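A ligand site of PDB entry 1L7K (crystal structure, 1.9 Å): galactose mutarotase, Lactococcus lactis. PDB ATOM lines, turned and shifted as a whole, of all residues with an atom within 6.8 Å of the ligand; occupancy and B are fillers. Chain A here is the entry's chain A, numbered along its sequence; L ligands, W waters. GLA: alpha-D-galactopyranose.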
ATOM      1  N   ASP A  58      32.884 -12.538  20.684  1.00  0.00           N
ATOM      2  CA  ASP A  58      31.471 -12.696  20.901  1.00  0.00           C
ATOM      3  C   ASP A  58      31.332 -13.881  21.799  1.00  0.00           C
ATOM      4  O   ASP A  58      31.668 -15.013  21.398  1.00  0.00           O
ATOM      5  CB  ASP A  58      30.670 -12.901  19.586  1.00  0.00           C
ATOM      6  CG  ASP A  58      29.175 -13.056  19.839  1.00  0.00           C
ATOM      7  OD1 ASP A  58      28.664 -13.008  20.958  1.00  0.00           O
ATOM      8  OD2 ASP A  58      28.455 -13.255  18.749  1.00  0.00           O
ATOM      9  N   TYR A  60      28.564 -15.185  23.045  1.00  0.00           N
ATOM     10  CA  TYR A  60      27.358 -15.979  23.030  1.00  0.00           C
ATOM     11  C   TYR A  60      27.370 -17.311  22.264  1.00  0.00           C
ATOM     12  O   TYR A  60      26.717 -18.309  22.650  1.00  0.00           O
ATOM     13  CB  TYR A  60      26.125 -15.120  22.649  1.00  0.00           C
ATOM     14  CG  TYR A  60      25.754 -14.015  23.656  1.00  0.00           C
ATOM     15  CD1 TYR A  60      25.824 -12.662  23.304  1.00  0.00           C
ATOM     16  CD2 TYR A  60      25.333 -14.315  24.942  1.00  0.00           C
ATOM     17  CE1 TYR A  60      25.507 -11.654  24.217  1.00  0.00           C
ATOM     18  CE2 TYR A  60      25.018 -13.323  25.874  1.00  0.00           C
ATOM     19  CZ  TYR A  60      25.081 -11.976  25.501  1.00  0.00           C
ATOM     20  OH  TYR A  60      24.755 -10.998  26.416  1.00  0.00           O
ATOM     21  N   PRO A  61      28.090 -17.341  21.142  1.00  0.00           N
ATOM     22  CA  PRO A  61      28.078 -18.549  20.318  1.00  0.00           C
ATOM     23  C   PRO A  61      28.343 -19.866  21.044  1.00  0.00           C
ATOM     24  O   PRO A  61      29.388 -20.062  21.657  1.00  0.00           O
ATOM     25  CB  PRO A  61      29.080 -18.305  19.180  1.00  0.00           C
ATOM     26  CG  PRO A  61      29.344 -16.824  19.147  1.00  0.00           C
ATOM     27  CD  PRO A  61      28.825 -16.242  20.473  1.00  0.00           C
ATOM     28  N   GLY A  70      17.040 -14.250  26.485  1.00  0.00           N
ATOM     29  CA  GLY A  70      16.211 -13.262  25.811  1.00  0.00           C
ATOM     30  C   GLY A  70      16.211 -11.897  26.474  1.00  0.00           C
ATOM     31  O   GLY A  70      16.958 -11.644  27.420  1.00  0.00           O
ATOM     32  N   ARG A  71      15.358 -11.026  25.941  1.00  0.00           N
ATOM     33  CA  ARG A  71      15.252  -9.693  26.456  1.00  0.00           C
ATOM     34  C   ARG A  71      14.087  -9.504  27.393  1.00  0.00           C
ATOM     35  O   ARG A  71      12.927  -9.878  27.077  1.00  0.00           O
ATOM     36  CB  ARG A  71      15.062  -8.665  25.372  1.00  0.00           C
ATOM     37  CG  ARG A  71      16.169  -8.673  24.369  1.00  0.00           C
ATOM     38  CD  ARG A  71      15.991  -7.656  23.214  1.00  0.00           C
ATOM     39  NE  ARG A  71      17.291  -7.557  22.508  1.00  0.00           N
ATOM     40  CZ  ARG A  71      17.726  -8.430  21.586  1.00  0.00           C
ATOM     41  NH1 ARG A  71      17.012  -9.483  21.110  1.00  0.00           N
ATOM     42  NH2 ARG A  71      18.936  -8.191  21.096  1.00  0.00           N
ATOM     43  N   GLU A  90      21.578  -3.838  28.005  1.00  0.00           N
ATOM     44  CA  GLU A  90      21.305  -3.463  26.619  1.00  0.00           C
ATOM     45  C   GLU A  90      20.344  -2.335  26.743  1.00  0.00           C
ATOM     46  O   GLU A  90      19.127  -2.546  26.723  1.00  0.00           O
ATOM     47  CB  GLU A  90      20.648  -4.558  25.825  1.00  0.00           C
ATOM     48  CG  GLU A  90      20.823  -4.325  24.341  1.00  0.00           C
ATOM     49  CD  GLU A  90      19.933  -5.260  23.566  1.00  0.00           C
ATOM     50  OE1 GLU A  90      18.760  -5.470  23.836  1.00  0.00           O
ATOM     51  OE2 GLU A  90      20.540  -5.838  22.576  1.00  0.00           O
ATOM     52  N   LEU A  95      19.361  -8.401  28.807  1.00  0.00           N
ATOM     53  CA  LEU A  95      19.482  -9.366  27.727  1.00  0.00           C
ATOM     54  C   LEU A  95      20.326 -10.582  28.154  1.00  0.00           C
ATOM     55  O   LEU A  95      21.445 -10.446  28.609  1.00  0.00           O
ATOM     56  CB  LEU A  95      20.162  -8.703  26.504  1.00  0.00           C
ATOM     57  CG  LEU A  95      20.713  -9.688  25.433  1.00  0.00           C
ATOM     58  CD1 LEU A  95      19.616 -10.366  24.600  1.00  0.00           C
ATOM     59  CD2 LEU A  95      21.694  -8.961  24.534  1.00  0.00           C
ATOM     60  N   HIS A  96      19.827 -11.784  27.995  1.00  0.00           N
ATOM     61  CA  HIS A  96      20.594 -12.986  28.354  1.00  0.00           C
ATOM     62  C   HIS A  96      21.171 -12.985  29.767  1.00  0.00           C
ATOM     63  O   HIS A  96      22.350 -13.356  29.963  1.00  0.00           O
ATOM     64  CB  HIS A  96      21.732 -13.237  27.355  1.00  0.00           C
ATOM     65  CG  HIS A  96      21.193 -13.536  25.983  1.00  0.00           C
ATOM     66  ND1 HIS A  96      19.924 -14.143  25.833  1.00  0.00           N
ATOM     67  CD2 HIS A  96      21.738 -13.343  24.756  1.00  0.00           C
ATOM     68  CE1 HIS A  96      19.748 -14.293  24.531  1.00  0.00           C
ATOM     69  NE2 HIS A  96      20.809 -13.808  23.849  1.00  0.00           N
ATOM     70  N   HIS A 170      22.789 -21.486  22.979  1.00  0.00           N
ATOM     71  CA  HIS A 170      22.945 -20.554  21.889  1.00  0.00           C
ATOM     72  C   HIS A 170      23.852 -20.985  20.713  1.00  0.00           C
ATOM     73  O   HIS A 170      24.610 -20.186  20.150  1.00  0.00           O
ATOM     74  CB  HIS A 170      23.404 -19.215  22.468  1.00  0.00           C
ATOM     75  CG  HIS A 170      22.974 -18.002  21.666  1.00  0.00           C
ATOM     76  ND1 HIS A 170      23.565 -17.679  20.460  1.00  0.00           N
ATOM     77  CD2 HIS A 170      22.020 -17.061  21.931  1.00  0.00           C
ATOM     78  CE1 HIS A 170      22.976 -16.584  20.020  1.00  0.00           C
ATOM     79  NE2 HIS A 170      22.051 -16.184  20.890  1.00  0.00           N
ATOM     80  N   TYR A 172      24.998 -21.790  16.912  1.00  0.00           N
ATOM     81  CA  TYR A 172      24.660 -21.265  15.596  1.00  0.00           C
ATOM     82  C   TYR A 172      25.011 -22.348  14.566  1.00  0.00           C
ATOM     83  O   TYR A 172      26.157 -22.810  14.492  1.00  0.00           O
ATOM     84  CB  TYR A 172      25.539 -20.054  15.162  1.00  0.00           C
ATOM     85  CG  TYR A 172      25.214 -18.723  15.793  1.00  0.00           C
ATOM     86  CD1 TYR A 172      25.836 -18.297  16.970  1.00  0.00           C
ATOM     87  CD2 TYR A 172      24.311 -17.867  15.175  1.00  0.00           C
ATOM     88  CE1 TYR A 172      25.545 -17.049  17.521  1.00  0.00           C
ATOM     89  CE2 TYR A 172      24.002 -16.618  15.712  1.00  0.00           C
ATOM     90  CZ  TYR A 172      24.621 -16.200  16.893  1.00  0.00           C
ATOM     91  OH  TYR A 172      24.319 -14.966  17.427  1.00  0.00           O
ATOM     92  N   GLU A 203      13.913  -4.318  20.070  1.00  0.00           N
ATOM     93  CA  GLU A 203      13.609  -5.723  20.053  1.00  0.00           C
ATOM     94  C   GLU A 203      12.809  -6.246  21.191  1.00  0.00           C
ATOM     95  O   GLU A 203      12.783  -7.460  21.395  1.00  0.00           O
ATOM     96  CB  GLU A 203      14.771  -6.648  19.642  1.00  0.00           C
ATOM     97  CG  GLU A 203      15.428  -6.213  18.301  1.00  0.00           C
ATOM     98  CD  GLU A 203      16.812  -6.804  17.986  1.00  0.00           C
ATOM     99  OE1 GLU A 203      17.837  -6.136  17.968  1.00  0.00           O
ATOM    100  OE2 GLU A 203      16.771  -8.078  17.686  1.00  0.00           O
ATOM    101  N   VAL A 239      14.228  -6.158  11.307  1.00  0.00           N
ATOM    102  CA  VAL A 239      15.432  -6.747  11.859  1.00  0.00           C
ATOM    103  C   VAL A 239      16.479  -7.199  10.847  1.00  0.00           C
ATOM    104  O   VAL A 239      17.623  -7.534  11.201  1.00  0.00           O
ATOM    105  CB  VAL A 239      14.946  -7.859  12.786  1.00  0.00           C
ATOM    106  CG1 VAL A 239      14.939  -9.237  12.139  1.00  0.00           C
ATOM    107  CG2 VAL A 239      15.620  -7.798  14.135  1.00  0.00           C
ATOM    108  N   ASP A 243      14.621 -12.846  13.875  1.00  0.00           N
ATOM    109  CA  ASP A 243      15.051 -12.642  15.271  1.00  0.00           C
ATOM    110  C   ASP A 243      13.810 -12.694  16.115  1.00  0.00           C
ATOM    111  O   ASP A 243      13.484 -11.721  16.778  1.00  0.00           O
ATOM    112  CB  ASP A 243      15.797 -11.305  15.520  1.00  0.00           C
ATOM    113  CG  ASP A 243      16.649 -11.396  16.765  1.00  0.00           C
ATOM    114  OD1 ASP A 243      16.666 -12.387  17.476  1.00  0.00           O
ATOM    115  OD2 ASP A 243      17.404 -10.339  16.966  1.00  0.00           O
ATOM    116  N   HIS A 244      13.120 -13.860  16.046  1.00  0.00           N
ATOM    117  CA  HIS A 244      11.850 -14.043  16.694  1.00  0.00           C
ATOM    118  C   HIS A 244      11.528 -15.400  17.260  1.00  0.00           C
ATOM    119  O   HIS A 244      11.954 -16.445  16.770  1.00  0.00           O
ATOM    120  CB  HIS A 244      10.748 -13.895  15.591  1.00  0.00           C
ATOM    121  CG  HIS A 244      10.746 -12.560  14.910  1.00  0.00           C
ATOM    122  ND1 HIS A 244      11.721 -12.202  13.960  1.00  0.00           N
ATOM    123  CD2 HIS A 244       9.876 -11.512  15.044  1.00  0.00           C
ATOM    124  CE1 HIS A 244      11.458 -10.953  13.563  1.00  0.00           C
ATOM    125  NE2 HIS A 244      10.350 -10.523  14.195  1.00  0.00           N
ATOM    126  N   VAL A 277      13.283 -19.689  19.559  1.00  0.00           N
ATOM    127  CA  VAL A 277      13.683 -18.396  19.082  1.00  0.00           C
ATOM    128  C   VAL A 277      14.658 -18.583  17.942  1.00  0.00           C
ATOM    129  O   VAL A 277      15.682 -19.254  18.077  1.00  0.00           O
ATOM    130  CB  VAL A 277      14.296 -17.568  20.184  1.00  0.00           C
ATOM    131  CG1 VAL A 277      14.914 -16.299  19.559  1.00  0.00           C
ATOM    132  CG2 VAL A 277      13.173 -17.180  21.165  1.00  0.00           C
ATOM    133  N   ILE A 278      14.347 -18.015  16.807  1.00  0.00           N
ATOM    134  CA  ILE A 278      15.266 -18.192  15.691  1.00  0.00           C
ATOM    135  C   ILE A 278      15.953 -16.902  15.316  1.00  0.00           C
ATOM    136  O   ILE A 278      15.260 -15.936  15.016  1.00  0.00           O
ATOM    137  CB  ILE A 278      14.525 -18.701  14.455  1.00  0.00           C
ATOM    138  CG1 ILE A 278      13.836 -20.005  14.770  1.00  0.00           C
ATOM    139  CG2 ILE A 278      15.503 -18.872  13.274  1.00  0.00           C
ATOM    140  CD1 ILE A 278      13.289 -20.690  13.520  1.00  0.00           C
ATOM    141  N   PHE A 279      17.291 -16.901  15.365  1.00  0.00           N
ATOM    142  CA  PHE A 279      18.047 -15.688  15.009  1.00  0.00           C
ATOM    143  C   PHE A 279      19.021 -16.016  13.867  1.00  0.00           C
ATOM    144  O   PHE A 279      19.877 -16.922  13.997  1.00  0.00           O
ATOM    145  CB  PHE A 279      18.801 -15.174  16.243  1.00  0.00           C
ATOM    146  CG  PHE A 279      19.802 -14.064  15.987  1.00  0.00           C
ATOM    147  CD1 PHE A 279      19.415 -12.846  15.429  1.00  0.00           C
ATOM    148  CD2 PHE A 279      21.139 -14.252  16.354  1.00  0.00           C
ATOM    149  CE1 PHE A 279      20.334 -11.812  15.245  1.00  0.00           C
ATOM    150  CE2 PHE A 279      22.076 -13.249  16.142  1.00  0.00           C
ATOM    151  CZ  PHE A 279      21.669 -12.012  15.607  1.00  0.00           C
ATOM    152  N   THR A 280      18.898 -15.300  12.766  1.00  0.00           N
ATOM    153  CA  THR A 280      19.744 -15.529  11.569  1.00  0.00           C
ATOM    154  C   THR A 280      21.024 -14.678  11.432  1.00  0.00           C
ATOM    155  O   THR A 280      21.398 -14.295  10.324  1.00  0.00           O
ATOM    156  CB  THR A 280      18.892 -15.435  10.279  1.00  0.00           C
ATOM    157  OG1 THR A 280      18.221 -14.190  10.271  1.00  0.00           O
ATOM    158  CG2 THR A 280      17.878 -16.546  10.303  1.00  0.00           C
ATOM    159  N   PHE A 283      24.118  -9.625  11.466  1.00  0.00           N
ATOM    160  CA  PHE A 283      25.206  -8.704  11.855  1.00  0.00           C
ATOM    161  C   PHE A 283      25.689  -7.685  10.816  1.00  0.00           C
ATOM    162  O   PHE A 283      26.628  -6.912  11.041  1.00  0.00           O
ATOM    163  CB  PHE A 283      26.400  -9.436  12.494  1.00  0.00           C
ATOM    164  CG  PHE A 283      25.995 -10.308  13.681  1.00  0.00           C
ATOM    165  CD1 PHE A 283      26.180 -11.693  13.659  1.00  0.00           C
ATOM    166  CD2 PHE A 283      25.466  -9.719  14.825  1.00  0.00           C
ATOM    167  CE1 PHE A 283      25.830 -12.485  14.758  1.00  0.00           C
ATOM    168  CE2 PHE A 283      25.096 -10.501  15.929  1.00  0.00           C
ATOM    169  CZ  PHE A 283      25.276 -11.882  15.883  1.00  0.00           C
ATOM    170  N   THR A 302      20.303 -19.762  14.709  1.00  0.00           N
ATOM    171  CA  THR A 302      20.116 -20.437  15.965  1.00  0.00           C
ATOM    172  C   THR A 302      18.763 -21.128  16.078  1.00  0.00           C
ATOM    173  O   THR A 302      17.825 -20.875  15.348  1.00  0.00           O
ATOM    174  CB  THR A 302      20.115 -19.398  17.142  1.00  0.00           C
ATOM    175  OG1 THR A 302      19.029 -18.488  16.992  1.00  0.00           O
ATOM    176  CG2 THR A 302      21.420 -18.610  17.234  1.00  0.00           C
ATOM    177  N   GLU A 304      17.040 -21.406  19.515  1.00  0.00           N
ATOM    178  CA  GLU A 304      17.056 -21.269  20.988  1.00  0.00           C
ATOM    179  C   GLU A 304      15.754 -21.794  21.592  1.00  0.00           C
ATOM    180  O   GLU A 304      14.738 -21.133  21.550  1.00  0.00           O
ATOM    181  CB  GLU A 304      17.315 -19.803  21.348  1.00  0.00           C
ATOM    182  CG  GLU A 304      18.546 -19.253  20.573  1.00  0.00           C
ATOM    183  CD  GLU A 304      18.767 -17.786  20.764  1.00  0.00           C
ATOM    184  OE1 GLU A 304      18.709 -17.212  21.831  1.00  0.00           O
ATOM    185  OE2 GLU A 304      19.014 -17.176  19.631  1.00  0.00           O
HETATM  186  C1  GLA L   1      19.559 -13.769  20.456  1.00  0.00           C
HETATM  187  C2  GLA L   1      18.892 -12.408  20.208  1.00  0.00           C
HETATM  188  C3  GLA L   1      19.623 -11.605  19.145  1.00  0.00           C
HETATM  189  C4  GLA L   1      21.067 -11.407  19.619  1.00  0.00           C
HETATM  190  C5  GLA L   1      21.689 -12.787  19.994  1.00  0.00           C
HETATM  191  C6  GLA L   1      23.071 -12.723  20.612  1.00  0.00           C
HETATM  192  O1  GLA L   1      19.630 -14.536  19.248  1.00  0.00           O
HETATM  193  O2  GLA L   1      17.500 -12.478  19.867  1.00  0.00           O
HETATM  194  O3  GLA L   1      18.941 -10.327  18.989  1.00  0.00           O
HETATM  195  O4  GLA L   1      21.194 -10.476  20.690  1.00  0.00           O
HETATM  196  O5  GLA L   1      20.898 -13.522  20.943  1.00  0.00           O
HETATM  197  O6  GLA L   1      23.989 -12.073  19.745  1.00  0.00           O
HETATM  198  O   HOH W   1      20.272  -8.536  17.761  1.00  0.00           O
HETATM  199  O   HOH W   2      25.957  -9.939  20.383  1.00  0.00           O
HETATM  200  O   HOH W   3      26.005 -13.923  19.208  1.00  0.00           O
HETATM  201  O   HOH W   4      15.987 -13.644  22.217  1.00  0.00           O
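The side-chain hydroxyl of Thr 302 lies within hydrogen-bond range of the backbone NH of Phe 279, 2.9 Å away.
OE2 of Glu 304 lies within hydrogen-bond range of OG1 of Thr 302.
N of Asp 243 sits close to O of Ile 278 (3.4 Å).
O of Glu 304 lies within hydrogen-bond range of N of Val 277 (2.9 Å).
NH1 of Arg 71 lies within salt-bridge range of OE2 of Glu 203, 3.7 Å away.
The side-chain carboxylate (OE2) of Glu 203 sits close to the side-chain carboxylate (OD2) of Asp 243.
The side-chain carboxylate (OE2) of Glu 304 is in hydrogen-bond range of a ring nitrogen (NE2) of His 170.
The guanidinium group (NE) of Arg 71 lies within salt-bridge range of the side-chain carboxylate (OE1) of Glu 90, 2.9 Å away.
Water W1 lies within hydrogen-bond range of an oxygen (O3) of the ligand (2.5 Å), the side-chain carboxylate of Glu 203 (3.4 Å) and the side-chain carboxylate of Asp 243 (3.5 Å).
Water W3 lies within hydrogen-bond range of OD2 of Asp 58, OH of Tyr 172 and O6 of the ligand.
NE2 of His 96 is in hydrogen-bond range of O5 of the ligand (2.9 Å).
An oxygen (O1) of the ligand lies within hydrogen-bond range of the side-chain carboxylate of Glu 304.
The guanidinium group of Arg 71 sits at hydrogen-bond distance from an oxygen (O3) of the ligand (3.0 Å).
OE2 of Glu 203 is in hydrogen-bond range of O3 of the ligand, 3.4 Å away.
An oxygen (O2) of the ligand lies within hydrogen-bond range of the side-chain carboxylate (OD1) of Asp 243.
A ring nitrogen (NE2) of His 170 is in hydrogen-bond range of an oxygen (O5) of the ligand.
Tyr 60 touches the ligand.
Tyr 172 touches the ligand (OH to O6, 3.7 Å).
CB of Phe 279 touches O1 of the ligand, at 3.2 Å.
The nearest printed residue that does not touch the ligand is Phe 283 (4.1 Å).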
